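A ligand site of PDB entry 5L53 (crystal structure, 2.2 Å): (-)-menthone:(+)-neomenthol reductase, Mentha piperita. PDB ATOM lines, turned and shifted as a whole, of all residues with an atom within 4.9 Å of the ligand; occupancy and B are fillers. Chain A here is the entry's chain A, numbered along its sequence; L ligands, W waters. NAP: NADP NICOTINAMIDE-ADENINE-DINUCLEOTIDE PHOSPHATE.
N of Arg 47 lies close to O of Leu 76 (3.4 Å). The side-chain amide nitrogen (ND2) of Asn 104 sits at hydrogen-bond distance from the backbone carbonyl oxygen (O) of Gly 22, 3.0 Å away. The side-chain carboxylate (OD1) of Asp 77 is in hydrogen-bond range of the backbone NH (N) of Ala 79. The backbone carbonyl oxygen (O) of Val 188 lies within hydrogen-bond range of the side-chain amino group (NZ) of Lys 250.
CA of Gly 26 touches O2N of the ligand (3.5 Å). Leu 76 touches the ligand. Ala 105 touches the ligand (CB to N3A, 3.4 Å). OG1 of Thr 161 touches N6A of the ligand, at 3.6 Å. Val 188 touches the ligand (CG1 to O4D, 3.1 Å). Ser 189 touches the ligand. Ser 190 touches the ligand. CD of Pro 274 touches C6N of the ligand (3.6 Å). Hydrophobic or aromatic side chains that line the ligand: Val 78, Ala 105, Val 188, Tyr 246 and Pro 274.
The guanidinium group (NH2) of Arg 47 lies within salt-bridge range of an oxygen (O3X) of the ligand (2.7 Å). OH of Tyr 246 sits at hydrogen-bond distance from O2D of the ligand, at 2.7 Å. The backbone carbonyl oxygen (O) of Asn 104 is in hydrogen-bond range of an oxygen (O3D) of the ligand. The side-chain carboxylate (OD1) of Asp 77 is in hydrogen-bond range of a nitrogen (N6A) of the ligand. The backbone NH (N) of Val 78 lies within hydrogen-bond range of a nitrogen (N1A) of the ligand. The side-chain amino group (NZ) of Lys 250 sits at hydrogen-bond distance from an oxygen (O3D) of the ligand (3.1 Å). An oxygen (O1X) of the ligand is in hydrogen-bond range of the side-chain amide nitrogen (ND2) of Asn 24 (3.2 Å). N of Ile 27 is in hydrogen-bond range of O2N of the ligand (3.2 Å). The backbone carbonyl oxygen (O) of Gly 22 lies within hydrogen-bond range of an oxygen (O3B) of the ligand (3.2 Å). NZ of Lys 25 lies within salt-bridge range of O1X of the ligand. N of Gly 106 is in hydrogen-bond range of O4B of the ligand, at 3.4 Å.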
ATOM      1  N   GLY A  22     -30.860  26.963  14.930  1.00  0.00           N
ATOM      2  CA  GLY A  22     -30.324  27.284  16.254  1.00  0.00           C
ATOM      3  C   GLY A  22     -30.882  28.584  16.828  1.00  0.00           C
ATOM      4  O   GLY A  22     -30.114  29.454  17.274  1.00  0.00           O
ATOM      5  N   ALA A  23     -32.204  28.744  16.817  1.00  0.00           N
ATOM      6  CA  ALA A  23     -32.796  30.053  17.046  1.00  0.00           C
ATOM      7  C   ALA A  23     -33.488  30.215  18.394  1.00  0.00           C
ATOM      8  O   ALA A  23     -34.150  31.243  18.606  1.00  0.00           O
ATOM      9  CB  ALA A  23     -33.784  30.379  15.922  1.00  0.00           C
ATOM     10  N   ASN A  24     -33.334  29.259  19.337  1.00  0.00           N
ATOM     11  CA  ASN A  24     -33.932  29.366  20.665  1.00  0.00           C
ATOM     12  C   ASN A  24     -33.148  30.235  21.643  1.00  0.00           C
ATOM     13  O   ASN A  24     -33.630  30.489  22.742  1.00  0.00           O
ATOM     14  CB  ASN A  24     -34.139  27.974  21.291  1.00  0.00           C
ATOM     15  CG  ASN A  24     -32.832  27.174  21.384  1.00  0.00           C
ATOM     16  OD1 ASN A  24     -32.358  26.604  20.376  1.00  0.00           O
ATOM     17  ND2 ASN A  24     -32.251  27.120  22.579  1.00  0.00           N
ATOM     18  N   LYS A  25     -31.948  30.702  21.284  1.00  0.00           N
ATOM     19  CA  LYS A  25     -31.199  31.613  22.152  1.00  0.00           C
ATOM     20  C   LYS A  25     -30.184  32.360  21.317  1.00  0.00           C
ATOM     21  O   LYS A  25     -30.034  32.106  20.118  1.00  0.00           O
ATOM     22  CB  LYS A  25     -30.514  30.862  23.309  1.00  0.00           C
ATOM     23  CG  LYS A  25     -29.430  29.836  22.846  1.00  0.00           C
ATOM     24  CD  LYS A  25     -28.767  29.120  24.018  1.00  0.00           C
ATOM     25  CE  LYS A  25     -27.739  28.115  23.568  1.00  0.00           C
ATOM     26  NZ  LYS A  25     -27.177  27.395  24.729  1.00  0.00           N
ATOM     27  N   GLY A  26     -29.485  33.295  21.954  1.00  0.00           N
ATOM     28  CA  GLY A  26     -28.307  33.879  21.319  1.00  0.00           C
ATOM     29  C   GLY A  26     -28.669  34.795  20.173  1.00  0.00           C
ATOM     30  O   GLY A  26     -29.676  35.488  20.198  1.00  0.00           O
ATOM     31  N   ILE A  27     -27.835  34.774  19.126  1.00  0.00           N
ATOM     32  CA  ILE A  27     -28.078  35.652  17.973  1.00  0.00           C
ATOM     33  C   ILE A  27     -29.250  35.134  17.135  1.00  0.00           C
ATOM     34  O   ILE A  27     -30.059  35.931  16.629  1.00  0.00           O
ATOM     35  CB  ILE A  27     -26.805  35.765  17.126  1.00  0.00           C
ATOM     36  CG1 ILE A  27     -25.676  36.313  18.001  1.00  0.00           C
ATOM     37  CG2 ILE A  27     -27.070  36.702  15.986  1.00  0.00           C
ATOM     38  CD1 ILE A  27     -24.303  36.168  17.403  1.00  0.00           C
ATOM     39  N   GLY A  28     -29.345  33.810  16.949  1.00  0.00           N
ATOM     40  CA  GLY A  28     -30.484  33.232  16.246  1.00  0.00           C
ATOM     41  C   GLY A  28     -31.812  33.772  16.735  1.00  0.00           C
ATOM     42  O   GLY A  28     -32.634  34.232  15.928  1.00  0.00           O
ATOM     43  N   ARG A  47     -32.828  22.726  18.517  1.00  0.00           N
ATOM     44  CA  ARG A  47     -32.473  21.331  18.670  1.00  0.00           C
ATOM     45  C   ARG A  47     -33.436  20.625  19.631  1.00  0.00           C
ATOM     46  O   ARG A  47     -33.905  19.509  19.361  1.00  0.00           O
ATOM     47  CB  ARG A  47     -31.028  21.227  19.114  1.00  0.00           C
ATOM     48  CG  ARG A  47     -30.615  19.801  19.238  1.00  0.00           C
ATOM     49  CD  ARG A  47     -29.121  19.678  19.199  1.00  0.00           C
ATOM     50  NE  ARG A  47     -28.485  20.686  20.030  1.00  0.00           N
ATOM     51  CZ  ARG A  47     -27.197  20.648  20.388  1.00  0.00           C
ATOM     52  NH1 ARG A  47     -26.441  19.629  20.009  1.00  0.00           N
ATOM     53  NH2 ARG A  47     -26.682  21.634  21.141  1.00  0.00           N
ATOM     54  N   ASP A  48     -33.802  21.298  20.718  1.00  0.00           N
ATOM     55  CA  ASP A  48     -34.782  20.777  21.672  1.00  0.00           C
ATOM     56  C   ASP A  48     -36.159  21.401  21.450  1.00  0.00           C
ATOM     57  O   ASP A  48     -36.294  22.632  21.458  1.00  0.00           O
ATOM     58  CB  ASP A  48     -34.328  21.058  23.109  1.00  0.00           C
ATOM     59  CG  ASP A  48     -35.326  20.531  24.128  1.00  0.00           C
ATOM     60  OD1 ASP A  48     -35.994  21.345  24.809  1.00  0.00           O
ATOM     61  OD2 ASP A  48     -35.467  19.277  24.197  1.00  0.00           O
ATOM     62  N   ARG A  51     -37.465  23.947  24.333  1.00  0.00           N
ATOM     63  CA  ARG A  51     -36.838  25.262  24.442  1.00  0.00           C
ATOM     64  C   ARG A  51     -37.274  26.184  23.317  1.00  0.00           C
ATOM     65  O   ARG A  51     -37.413  27.399  23.523  1.00  0.00           O
ATOM     66  CB  ARG A  51     -35.325  25.131  24.516  1.00  0.00           C
ATOM     67  CG  ARG A  51     -34.931  24.101  25.554  1.00  0.00           C
ATOM     68  CD  ARG A  51     -33.455  23.992  25.768  1.00  0.00           C
ATOM     69  NE  ARG A  51     -32.810  25.287  25.600  1.00  0.00           N
ATOM     70  CZ  ARG A  51     -32.562  26.175  26.584  1.00  0.00           C
ATOM     71  NH1 ARG A  51     -32.890  25.914  27.844  1.00  0.00           N
ATOM     72  NH2 ARG A  51     -31.968  27.333  26.277  1.00  0.00           N
ATOM     73  N   LEU A  76     -35.495  20.977  15.276  1.00  0.00           N
ATOM     74  CA  LEU A  76     -34.539  20.778  14.183  1.00  0.00           C
ATOM     75  C   LEU A  76     -33.180  20.478  14.781  1.00  0.00           C
ATOM     76  O   LEU A  76     -32.606  21.336  15.459  1.00  0.00           O
ATOM     77  CB  LEU A  76     -34.410  22.003  13.239  1.00  0.00           C
ATOM     78  CG  LEU A  76     -33.323  21.780  12.187  1.00  0.00           C
ATOM     79  CD1 LEU A  76     -33.738  20.597  11.202  1.00  0.00           C
ATOM     80  CD2 LEU A  76     -33.009  23.044  11.416  1.00  0.00           C
ATOM     81  N   ASP A  77     -32.659  19.304  14.502  1.00  0.00           N
ATOM     82  CA  ASP A  77     -31.260  18.980  14.744  1.00  0.00           C
ATOM     83  C   ASP A  77     -30.583  18.817  13.387  1.00  0.00           C
ATOM     84  O   ASP A  77     -30.858  17.834  12.672  1.00  0.00           O
ATOM     85  CB  ASP A  77     -31.133  17.703  15.575  1.00  0.00           C
ATOM     86  CG  ASP A  77     -29.711  17.389  15.947  1.00  0.00           C
ATOM     87  OD1 ASP A  77     -28.789  17.942  15.277  1.00  0.00           O
ATOM     88  OD2 ASP A  77     -29.515  16.590  16.888  1.00  0.00           O
ATOM     89  N   VAL A  78     -29.670  19.745  13.067  1.00  0.00           N
ATOM     90  CA  VAL A  78     -29.071  19.813  11.727  1.00  0.00           C
ATOM     91  C   VAL A  78     -28.169  18.605  11.466  1.00  0.00           C
ATOM     92  O   VAL A  78     -27.838  18.332  10.303  1.00  0.00           O
ATOM     93  CB  VAL A  78     -28.261  21.112  11.509  1.00  0.00           C
ATOM     94  CG1 VAL A  78     -29.096  22.294  11.839  1.00  0.00           C
ATOM     95  CG2 VAL A  78     -26.931  21.136  12.334  1.00  0.00           C
ATOM     96  N   ALA A  79     -27.779  17.883  12.508  1.00  0.00           N
ATOM     97  CA  ALA A  79     -26.939  16.708  12.404  1.00  0.00           C
ATOM     98  C   ALA A  79     -27.722  15.422  12.164  1.00  0.00           C
ATOM     99  O   ALA A  79     -27.100  14.358  12.040  1.00  0.00           O
ATOM    100  CB  ALA A  79     -26.112  16.521  13.672  1.00  0.00           C
ATOM    101  N   ASN A 104     -27.685  29.398  11.259  1.00  0.00           N
ATOM    102  CA  ASN A 104     -27.112  29.936  12.464  1.00  0.00           C
ATOM    103  C   ASN A 104     -26.668  28.875  13.453  1.00  0.00           C
ATOM    104  O   ASN A 104     -25.826  29.167  14.292  1.00  0.00           O
ATOM    105  CB  ASN A 104     -28.128  30.861  13.129  1.00  0.00           C
ATOM    106  CG  ASN A 104     -27.645  31.392  14.439  1.00  0.00           C
ATOM    107  OD1 ASN A 104     -26.795  32.297  14.481  1.00  0.00           O
ATOM    108  ND2 ASN A 104     -28.154  30.836  15.507  1.00  0.00           N
ATOM    109  N   ALA A 105     -27.217  27.660  13.371  1.00  0.00           N
ATOM    110  CA  ALA A 105     -26.802  26.620  14.306  1.00  0.00           C
ATOM    111  C   ALA A 105     -25.287  26.407  14.233  1.00  0.00           C
ATOM    112  O   ALA A 105     -24.736  26.314  13.140  1.00  0.00           O
ATOM    113  CB  ALA A 105     -27.554  25.319  14.003  1.00  0.00           C
ATOM    114  N   GLY A 106     -24.628  26.325  15.387  1.00  0.00           N
ATOM    115  CA  GLY A 106     -23.178  26.207  15.387  1.00  0.00           C
ATOM    116  C   GLY A 106     -22.600  25.797  16.722  1.00  0.00           C
ATOM    117  O   GLY A 106     -23.221  25.959  17.772  1.00  0.00           O
ATOM    118  N   LEU A 107     -21.395  25.242  16.659  1.00  0.00           N
ATOM    119  CA  LEU A 107     -20.623  24.760  17.795  1.00  0.00           C
ATOM    120  C   LEU A 107     -19.208  25.305  17.705  1.00  0.00           C
ATOM    121  O   LEU A 107     -18.678  25.475  16.603  1.00  0.00           O
ATOM    122  CB  LEU A 107     -20.488  23.237  17.821  1.00  0.00           C
ATOM    123  CG  LEU A 107     -21.703  22.517  18.283  1.00  0.00           C
ATOM    124  CD1 LEU A 107     -21.850  21.322  17.412  1.00  0.00           C
ATOM    125  CD2 LEU A 107     -21.417  22.119  19.689  1.00  0.00           C
ATOM    126  N   THR A 161     -21.593  19.529  12.688  1.00  0.00           N
ATOM    127  CA  THR A 161     -22.657  20.516  12.761  1.00  0.00           C
ATOM    128  C   THR A 161     -22.371  21.703  11.849  1.00  0.00           C
ATOM    129  O   THR A 161     -23.210  22.050  11.004  1.00  0.00           O
ATOM    130  CB  THR A 161     -22.845  21.010  14.200  1.00  0.00           C
ATOM    131  OG1 THR A 161     -23.429  19.988  15.004  1.00  0.00           O
ATOM    132  CG2 THR A 161     -23.738  22.279  14.269  1.00  0.00           C
ATOM    133  N   VAL A 188     -24.108  31.958   8.954  1.00  0.00           N
ATOM    134  CA  VAL A 188     -23.473  32.623  10.090  1.00  0.00           C
ATOM    135  C   VAL A 188     -22.112  31.977  10.339  1.00  0.00           C
ATOM    136  O   VAL A 188     -22.020  30.836  10.817  1.00  0.00           O
ATOM    137  CB  VAL A 188     -24.360  32.589  11.327  1.00  0.00           C
ATOM    138  CG1 VAL A 188     -23.694  33.308  12.500  1.00  0.00           C
ATOM    139  CG2 VAL A 188     -25.670  33.280  10.970  1.00  0.00           C
ATOM    140  N   SER A 189     -21.047  32.702   9.993  1.00  0.00           N
ATOM    141  CA  SER A 189     -19.645  32.288  10.107  1.00  0.00           C
ATOM    142  C   SER A 189     -18.997  32.968  11.332  1.00  0.00           C
ATOM    143  O   SER A 189     -19.700  33.363  12.273  1.00  0.00           O
ATOM    144  CB  SER A 189     -18.958  32.591   8.776  1.00  0.00           C
ATOM    145  OG  SER A 189     -17.768  31.847   8.594  1.00  0.00           O
ATOM    146  N   SER A 190     -17.669  33.134  11.309  1.00  0.00           N
ATOM    147  CA  SER A 190     -16.932  33.738  12.422  1.00  0.00           C
ATOM    148  C   SER A 190     -15.662  34.376  11.903  1.00  0.00           C
ATOM    149  O   SER A 190     -15.098  33.918  10.902  1.00  0.00           O
ATOM    150  CB  SER A 190     -16.565  32.704  13.494  1.00  0.00           C
ATOM    151  OG  SER A 190     -15.696  33.285  14.466  1.00  0.00           O
ATOM    152  N   TYR A 246     -13.051  24.586  14.989  1.00  0.00           N
ATOM    153  CA  TYR A 246     -13.874  25.733  14.675  1.00  0.00           C
ATOM    154  C   TYR A 246     -13.343  26.475  13.456  1.00  0.00           C
ATOM    155  O   TYR A 246     -14.090  26.764  12.515  1.00  0.00           O
ATOM    156  CB  TYR A 246     -13.925  26.647  15.874  1.00  0.00           C
ATOM    157  CG  TYR A 246     -14.974  27.730  15.788  1.00  0.00           C
ATOM    158  CD1 TYR A 246     -16.324  27.392  15.601  1.00  0.00           C
ATOM    159  CD2 TYR A 246     -14.634  29.066  15.970  1.00  0.00           C
ATOM    160  CE1 TYR A 246     -17.297  28.379  15.547  1.00  0.00           C
ATOM    161  CE2 TYR A 246     -15.608  30.060  15.939  1.00  0.00           C
ATOM    162  CZ  TYR A 246     -16.923  29.721  15.716  1.00  0.00           C
ATOM    163  OH  TYR A 246     -17.889  30.710  15.682  1.00  0.00           O
ATOM    164  N   LYS A 250     -15.457  26.558   9.930  1.00  0.00           N
ATOM    165  CA  LYS A 250     -16.067  27.794   9.452  1.00  0.00           C
ATOM    166  C   LYS A 250     -15.405  28.295   8.174  1.00  0.00           C
ATOM    167  O   LYS A 250     -16.091  28.845   7.298  1.00  0.00           O
ATOM    168  CB  LYS A 250     -16.033  28.855  10.544  1.00  0.00           C
ATOM    169  CG  LYS A 250     -16.907  28.554  11.736  1.00  0.00           C
ATOM    170  CD  LYS A 250     -18.380  28.755  11.405  1.00  0.00           C
ATOM    171  CE  LYS A 250     -19.206  28.795  12.629  1.00  0.00           C
ATOM    172  NZ  LYS A 250     -20.592  29.203  12.276  1.00  0.00           N
ATOM    173  N   CYS A 273     -19.826  37.383   9.464  1.00  0.00           N
ATOM    174  CA  CYS A 273     -19.378  37.361  10.857  1.00  0.00           C
ATOM    175  C   CYS A 273     -20.269  38.296  11.672  1.00  0.00           C
ATOM    176  O   CYS A 273     -20.333  39.495  11.361  1.00  0.00           O
ATOM    177  CB  CYS A 273     -17.915  37.769  11.012  1.00  0.00           C
ATOM    178  SG  CYS A 273     -17.506  38.069  12.793  1.00  0.00           S
ATOM    179  N   PRO A 274     -20.965  37.813  12.703  1.00  0.00           N
ATOM    180  CA  PRO A 274     -21.839  38.705  13.457  1.00  0.00           C
ATOM    181  C   PRO A 274     -21.034  39.496  14.490  1.00  0.00           C
ATOM    182  O   PRO A 274     -21.216  40.705  14.464  1.00  0.00           O
ATOM    183  CB  PRO A 274     -22.805  37.736  14.132  1.00  0.00           C
ATOM    184  CG  PRO A 274     -21.946  36.531  14.400  1.00  0.00           C
ATOM    185  CD  PRO A 274     -20.980  36.431  13.235  1.00  0.00           C
HETATM  186  PA  NAP L   1     -25.057  29.741  21.130  1.00  0.00           P
HETATM  187  O1A NAP L   1     -24.272  28.514  21.688  1.00  0.00           O
HETATM  188  O2A NAP L   1     -25.809  30.523  22.162  1.00  0.00           O
HETATM  189  O5B NAP L   1     -26.112  29.247  20.019  1.00  0.00           O
HETATM  190  C5B NAP L   1     -25.836  28.215  19.061  1.00  0.00           C
HETATM  191  C4B NAP L   1     -27.174  27.654  18.676  1.00  0.00           C
HETATM  192  O4B NAP L   1     -26.971  26.545  17.773  1.00  0.00           O
HETATM  193  C3B NAP L   1     -28.001  27.104  19.859  1.00  0.00           C
HETATM  194  O3B NAP L   1     -29.349  27.574  19.812  1.00  0.00           O
HETATM  195  C2B NAP L   1     -27.841  25.578  19.710  1.00  0.00           C
HETATM  196  O2B NAP L   1     -28.960  24.829  20.225  1.00  0.00           O
HETATM  197  C1B NAP L   1     -27.804  25.477  18.183  1.00  0.00           C
HETATM  198  N9A NAP L   1     -27.237  24.243  17.706  1.00  0.00           N
HETATM  199  C8A NAP L   1     -26.005  23.706  17.956  1.00  0.00           C
HETATM  200  N7A NAP L   1     -25.808  22.519  17.432  1.00  0.00           N
HETATM  201  C5A NAP L   1     -27.024  22.261  16.778  1.00  0.00           C
HETATM  202  C6A NAP L   1     -27.451  21.177  15.991  1.00  0.00           C
HETATM  203  N6A NAP L   1     -26.866  19.982  15.985  1.00  0.00           N
HETATM  204  N1A NAP L   1     -28.633  21.312  15.345  1.00  0.00           N
HETATM  205  C2A NAP L   1     -29.376  22.402  15.567  1.00  0.00           C
HETATM  206  N3A NAP L   1     -29.100  23.449  16.359  1.00  0.00           N
HETATM  207  C4A NAP L   1     -27.884  23.314  16.926  1.00  0.00           C
HETATM  208  O3  NAP L   1     -24.049  30.667  20.328  1.00  0.00           O
HETATM  209  PN  NAP L   1     -24.208  31.939  19.370  1.00  0.00           P
HETATM  210  O1N NAP L   1     -22.991  32.759  19.553  1.00  0.00           O
HETATM  211  O2N NAP L   1     -25.529  32.592  19.568  1.00  0.00           O
HETATM  212  O5D NAP L   1     -24.133  31.193  17.950  1.00  0.00           O
HETATM  213  C5D NAP L   1     -24.750  31.691  16.748  1.00  0.00           C
HETATM  214  C4D NAP L   1     -23.832  31.519  15.562  1.00  0.00           C
HETATM  215  O4D NAP L   1     -22.942  32.656  15.470  1.00  0.00           O
HETATM  216  C3D NAP L   1     -22.949  30.267  15.544  1.00  0.00           C
HETATM  217  O3D NAP L   1     -22.987  29.618  14.268  1.00  0.00           O
HETATM  218  C2D NAP L   1     -21.562  30.805  15.936  1.00  0.00           C
HETATM  219  O2D NAP L   1     -20.523  29.980  15.390  1.00  0.00           O
HETATM  220  C1D NAP L   1     -21.611  32.240  15.366  1.00  0.00           C
HETATM  221  N1N NAP L   1     -20.713  33.294  16.076  1.00  0.00           N
HETATM  222  C2N NAP L   1     -20.978  33.722  17.319  1.00  0.00           C
HETATM  223  C3N NAP L   1     -20.203  34.724  17.886  1.00  0.00           C
HETATM  224  C7N NAP L   1     -20.504  35.257  19.278  1.00  0.00           C
HETATM  225  O7N NAP L   1     -20.716  36.496  19.437  1.00  0.00           O
HETATM  226  N7N NAP L   1     -20.543  34.385  20.285  1.00  0.00           N
HETATM  227  C4N NAP L   1     -19.145  35.253  17.160  1.00  0.00           C
HETATM  228  C5N NAP L   1     -18.884  34.777  15.879  1.00  0.00           C
HETATM  229  C6N NAP L   1     -19.684  33.791  15.353  1.00  0.00           C
HETATM  230  P2B NAP L   1     -29.078  24.281  21.753  1.00  0.00           P
HETATM  231  O1X NAP L   1     -29.506  25.482  22.683  1.00  0.00           O
HETATM  232  O2X NAP L   1     -30.253  23.187  21.702  1.00  0.00           O
HETATM  233  O3X NAP L   1     -27.727  23.826  22.264  1.00  0.00           O
HETATM  234  O   HOH W   1     -27.957  31.578  18.187  1.00  0.00           O
